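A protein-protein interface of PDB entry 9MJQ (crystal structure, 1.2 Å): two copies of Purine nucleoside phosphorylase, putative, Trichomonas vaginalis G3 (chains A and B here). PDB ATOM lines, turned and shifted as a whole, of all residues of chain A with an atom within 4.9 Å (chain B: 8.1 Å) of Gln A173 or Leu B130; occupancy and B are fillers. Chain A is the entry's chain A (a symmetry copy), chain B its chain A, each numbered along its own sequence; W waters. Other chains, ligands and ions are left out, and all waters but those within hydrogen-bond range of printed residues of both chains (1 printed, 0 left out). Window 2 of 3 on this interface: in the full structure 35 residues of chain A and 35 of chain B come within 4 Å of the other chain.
NE2 of His B132 lies within hydrogen-bond range of OE2 of Glu A172, 2.7 Å away.
Of the 10 printed residues of chain B, 4 touch a printed residue of chain A. Hydrophobic or aromatic side chains of chain B within 4 Å of the printed part of chain A: Leu B129, Leu B130 and His B132. Along chain A the printed residues that touch a printed residue of chain B span positions 172 to 178.
Water W1 lies within hydrogen-bond range of OE1 of Glu A172 and NE2 of His B132.
Among the printed residues, merely in contact across the chains: Glu A172 with Leu B130, Gln A173 with Leu B130, Gly A174 with Leu B130, Leu A175 with Leu B130, Ala A178 with Arg B128, Ala A178 with Leu B129 and Ala A178 with Leu B130.
Gln A173 touches one residue of chain B. Leu B130 touches just these residues of chain A: Glu A172, Gln A173, Gly A174, Leu A175 and Ala A178. Gly A174 touches just one residue of chain B: Leu B130. Of the printed residues of chain B, Ala A178 touches Arg B128, Leu B129 and Leu B130. Of the printed residues of chain A, His B132 touches Glu A172 (2.7 Å). Printed residues of chain B within 4 Å of Glu A172: Leu B130 and His B132. Of the printed residues of chain A, Arg B128 touches Ala A178 (3.8 Å). Lys A171 touches none of the printed residues of chain B. Arg B126 touches none of the printed residues of chain A. The nearest residue of chain B that does not touch Gln A173 is His B132 (7.8 Å). The nearest printed residue of chain A that does not touch Arg B128 is Gly A174 (7.0 Å).
The side-chain amide oxygen (OD1) of Asn B125 is in hydrogen-bond range of the guanidinium group (NH1) of Arg B128 (2.9 Å).
No position is printed for both chains. Of the 8 pairs that touch across the chains among the printed residues, none has its exchanged pair printed and touching as well.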
ATOM      1  N   LYS A 171       1.113 -18.949  16.831  1.00  0.00           N
ATOM      2  CA  LYS A 171       2.354 -18.963  16.071  1.00  0.00           C
ATOM      3  C   LYS A 171       3.512 -18.540  16.965  1.00  0.00           C
ATOM      4  O   LYS A 171       4.559 -18.119  16.475  1.00  0.00           O
ATOM      5  CB  LYS A 171       2.225 -18.034  14.865  1.00  0.00           C
ATOM      6  CG  LYS A 171       1.126 -18.438  13.890  1.00  0.00           C
ATOM      7  CD  LYS A 171       0.795 -17.303  12.913  1.00  0.00           C
ATOM      8  CE  LYS A 171      -0.233 -17.716  11.876  1.00  0.00           C
ATOM      9  NZ  LYS A 171      -1.511 -18.116  12.524  1.00  0.00           N
ATOM     10  N   GLU A 172       3.336 -18.640  18.275  1.00  0.00           N
ATOM     11  CA  GLU A 172       4.206 -17.979  19.247  1.00  0.00           C
ATOM     12  C   GLU A 172       5.295 -18.926  19.732  1.00  0.00           C
ATOM     13  O   GLU A 172       5.058 -19.797  20.570  1.00  0.00           O
ATOM     14  CB  GLU A 172       3.360 -17.450  20.399  1.00  0.00           C
ATOM     15  CG  GLU A 172       4.128 -16.615  21.361  1.00  0.00           C
ATOM     16  CD  GLU A 172       3.268 -16.007  22.449  1.00  0.00           C
ATOM     17  OE1 GLU A 172       2.047 -16.279  22.506  1.00  0.00           O
ATOM     18  OE2 GLU A 172       3.850 -15.256  23.256  1.00  0.00           O
ATOM     19  N   GLN A 173       6.508 -18.717  19.241  1.00  0.00           N
ATOM     20  CA  GLN A 173       7.629 -19.548  19.647  1.00  0.00           C
ATOM     21  C   GLN A 173       7.911 -19.389  21.139  1.00  0.00           C
ATOM     22  O   GLN A 173       7.925 -18.280  21.681  1.00  0.00           O
ATOM     23  CB  GLN A 173       8.863 -19.158  18.837  1.00  0.00           C
ATOM     24  CG  GLN A 173       8.679 -19.247  17.331  1.00  0.00           C
ATOM     25  CD  GLN A 173       8.814 -20.656  16.792  1.00  0.00           C
ATOM     26  OE1 GLN A 173       8.960 -21.618  17.550  1.00  0.00           O
ATOM     27  NE2 GLN A 173       8.781 -20.785  15.469  1.00  0.00           N
ATOM     28  N   GLY A 174       8.125 -20.512  21.809  1.00  0.00           N
ATOM     29  CA  GLY A 174       8.475 -20.516  23.209  1.00  0.00           C
ATOM     30  C   GLY A 174       7.314 -20.507  24.175  1.00  0.00           C
ATOM     31  O   GLY A 174       7.536 -20.707  25.373  1.00  0.00           O
ATOM     32  N   LEU A 175       6.087 -20.275  23.706  1.00  0.00           N
ATOM     33  CA  LEU A 175       4.951 -20.202  24.615  1.00  0.00           C
ATOM     34  C   LEU A 175       4.717 -21.542  25.297  1.00  0.00           C
ATOM     35  O   LEU A 175       4.575 -21.610  26.522  1.00  0.00           O
ATOM     36  CB  LEU A 175       3.688 -19.751  23.879  1.00  0.00           C
ATOM     37  CG  LEU A 175       2.409 -19.704  24.739  1.00  0.00           C
ATOM     38  CD1 LEU A 175       2.466 -18.607  25.792  1.00  0.00           C
ATOM     39  CD2 LEU A 175       1.189 -19.534  23.871  1.00  0.00           C
ATOM     40  N   ALA A 178       7.249 -22.337  28.034  1.00  0.00           N
ATOM     41  CA  ALA A 178       7.062 -21.579  29.269  1.00  0.00           C
ATOM     42  C   ALA A 178       5.843 -22.066  30.041  1.00  0.00           C
ATOM     43  O   ALA A 178       5.897 -22.226  31.264  1.00  0.00           O
ATOM     44  CB  ALA A 178       6.961 -20.084  28.966  1.00  0.00           C
ATOM     45  N   ASN B 125       7.081 -11.649  36.739  1.00  0.00           N
ATOM     46  CA  ASN B 125       6.272 -12.727  36.189  1.00  0.00           C
ATOM     47  C   ASN B 125       6.010 -12.539  34.706  1.00  0.00           C
ATOM     48  O   ASN B 125       5.968 -13.529  33.964  1.00  0.00           O
ATOM     49  CB  ASN B 125       4.999 -12.893  37.015  1.00  0.00           C
ATOM     50  CG  ASN B 125       5.319 -13.283  38.428  1.00  0.00           C
ATOM     51  OD1 ASN B 125       6.339 -13.922  38.669  1.00  0.00           O
ATOM     52  ND2 ASN B 125       4.487 -12.883  39.372  1.00  0.00           N
ATOM     53  N   ARG B 126       5.917 -11.293  34.239  1.00  0.00           N
ATOM     54  CA  ARG B 126       5.897 -11.063  32.799  1.00  0.00           C
ATOM     55  C   ARG B 126       7.153 -11.632  32.164  1.00  0.00           C
ATOM     56  O   ARG B 126       7.108 -12.199  31.069  1.00  0.00           O
ATOM     57  CB  ARG B 126       5.753  -9.573  32.517  1.00  0.00           C
ATOM     58  CG  ARG B 126       4.414  -9.020  32.938  1.00  0.00           C
ATOM     59  CD  ARG B 126       4.252  -7.555  32.681  1.00  0.00           C
ATOM     60  NE  ARG B 126       3.016  -7.129  33.313  1.00  0.00           N
ATOM     61  CZ  ARG B 126       2.449  -5.949  33.149  1.00  0.00           C
ATOM     62  NH1 ARG B 126       2.999  -5.022  32.379  1.00  0.00           N
ATOM     63  NH2 ARG B 126       1.294  -5.701  33.753  1.00  0.00           N
ATOM     64  N   MET B 127       8.293 -11.487  32.840  1.00  0.00           N
ATOM     65  CA  MET B 127       9.533 -12.009  32.285  1.00  0.00           C
ATOM     66  C   MET B 127       9.523 -13.518  32.153  1.00  0.00           C
ATOM     67  O   MET B 127      10.243 -14.053  31.301  1.00  0.00           O
ATOM     68  CB  MET B 127      10.703 -11.570  33.150  1.00  0.00           C
ATOM     69  CG  MET B 127      10.952 -10.083  33.063  1.00  0.00           C
ATOM     70  SD  MET B 127      11.174  -9.472  31.377  1.00  0.00           S
ATOM     71  CE  MET B 127      12.588 -10.413  30.827  1.00  0.00           C
ATOM     72  N   ARG B 128       8.706 -14.217  32.949  1.00  0.00           N
ATOM     73  CA  ARG B 128       8.644 -15.668  32.926  1.00  0.00           C
ATOM     74  C   ARG B 128       7.686 -16.205  31.874  1.00  0.00           C
ATOM     75  O   ARG B 128       7.772 -17.390  31.523  1.00  0.00           O
ATOM     76  CB  ARG B 128       8.211 -16.192  34.301  1.00  0.00           C
ATOM     77  CG  ARG B 128       9.204 -15.948  35.399  1.00  0.00           C
ATOM     78  CD  ARG B 128       8.658 -16.340  36.778  1.00  0.00           C
ATOM     79  NE  ARG B 128       9.751 -16.399  37.753  1.00  0.00           N
ATOM     80  CZ  ARG B 128       9.939 -15.605  38.801  1.00  0.00           C
ATOM     81  NH1 ARG B 128       9.049 -14.695  39.164  1.00  0.00           N
ATOM     82  NH2 ARG B 128      11.051 -15.746  39.528  1.00  0.00           N
ATOM     83  N   LEU B 129       6.768 -15.382  31.370  1.00  0.00           N
ATOM     84  CA  LEU B 129       5.729 -15.868  30.466  1.00  0.00           C
ATOM     85  C   LEU B 129       5.602 -14.986  29.238  1.00  0.00           C
ATOM     86  O   LEU B 129       4.507 -14.596  28.840  1.00  0.00           O
ATOM     87  CB  LEU B 129       4.399 -16.030  31.200  1.00  0.00           C
ATOM     88  CG  LEU B 129       3.335 -16.872  30.497  1.00  0.00           C
ATOM     89  CD1 LEU B 129       3.861 -18.255  30.164  1.00  0.00           C
ATOM     90  CD2 LEU B 129       2.076 -16.970  31.336  1.00  0.00           C
ATOM     91  N   LEU B 130       6.740 -14.673  28.614  1.00  0.00           N
ATOM     92  CA  LEU B 130       6.778 -14.036  27.293  1.00  0.00           C
ATOM     93  C   LEU B 130       6.058 -12.694  27.296  1.00  0.00           C
ATOM     94  O   LEU B 130       5.526 -12.258  26.275  1.00  0.00           O
ATOM     95  CB  LEU B 130       6.220 -14.959  26.203  1.00  0.00           C
ATOM     96  CG  LEU B 130       7.072 -16.182  25.871  1.00  0.00           C
ATOM     97  CD1 LEU B 130       7.031 -17.230  26.966  1.00  0.00           C
ATOM     98  CD2 LEU B 130       6.640 -16.809  24.549  1.00  0.00           C
ATOM     99  N   GLY B 131       6.047 -12.019  28.439  1.00  0.00           N
ATOM    100  CA  GLY B 131       5.447 -10.715  28.574  1.00  0.00           C
ATOM    101  C   GLY B 131       3.974 -10.717  28.897  1.00  0.00           C
ATOM    102  O   GLY B 131       3.388  -9.635  29.040  1.00  0.00           O
ATOM    103  N   HIS B 132       3.368 -11.885  29.059  1.00  0.00           N
ATOM    104  CA  HIS B 132       1.937 -12.018  29.280  1.00  0.00           C
ATOM    105  C   HIS B 132       1.612 -11.983  30.775  1.00  0.00           C
ATOM    106  O   HIS B 132       2.482 -11.729  31.618  1.00  0.00           O
ATOM    107  CB  HIS B 132       1.443 -13.292  28.609  1.00  0.00           C
ATOM    108  CG  HIS B 132       1.807 -13.380  27.164  1.00  0.00           C
ATOM    109  ND1 HIS B 132       1.514 -12.379  26.255  1.00  0.00           N
ATOM    110  CD2 HIS B 132       2.440 -14.348  26.462  1.00  0.00           C
ATOM    111  CE1 HIS B 132       1.954 -12.733  25.062  1.00  0.00           C
ATOM    112  NE2 HIS B 132       2.524 -13.920  25.162  1.00  0.00           N
ATOM    113  N   ASP B 133       0.337 -12.203  31.101  1.00  0.00           N
ATOM    114  CA  ASP B 133      -0.143 -12.251  32.475  1.00  0.00           C
ATOM    115  C   ASP B 133      -0.006 -13.669  33.005  1.00  0.00           C
ATOM    116  O   ASP B 133      -0.703 -14.593  32.549  1.00  0.00           O
ATOM    117  CB  ASP B 133      -1.602 -11.827  32.614  1.00  0.00           C
ATOM    118  CG  ASP B 133      -1.828 -10.340  32.480  1.00  0.00           C
ATOM    119  OD1 ASP B 133      -0.887  -9.612  32.122  1.00  0.00           O
ATOM    120  OD2 ASP B 133      -2.962  -9.889  32.763  1.00  0.00           O
ATOM    121  N   PHE B 134       0.846 -13.809  34.003  1.00  0.00           N
ATOM    122  CA  PHE B 134       1.123 -15.062  34.695  1.00  0.00           C
ATOM    123  C   PHE B 134       0.601 -14.884  36.116  1.00  0.00           C
ATOM    124  O   PHE B 134       1.214 -14.145  36.897  1.00  0.00           O
ATOM    125  CB  PHE B 134       2.645 -15.247  34.688  1.00  0.00           C
ATOM    126  CG  PHE B 134       3.179 -16.501  35.374  1.00  0.00           C
ATOM    127  CD1 PHE B 134       2.444 -17.263  36.263  1.00  0.00           C
ATOM    128  CD2 PHE B 134       4.492 -16.865  35.139  1.00  0.00           C
ATOM    129  CE1 PHE B 134       3.017 -18.380  36.888  1.00  0.00           C
ATOM    130  CE2 PHE B 134       5.067 -17.949  35.766  1.00  0.00           C
ATOM    131  CZ  PHE B 134       4.324 -18.720  36.635  1.00  0.00           C
HETATM  132  O   HOH W   1      -0.004 -16.193  24.385  1.00  0.00           O
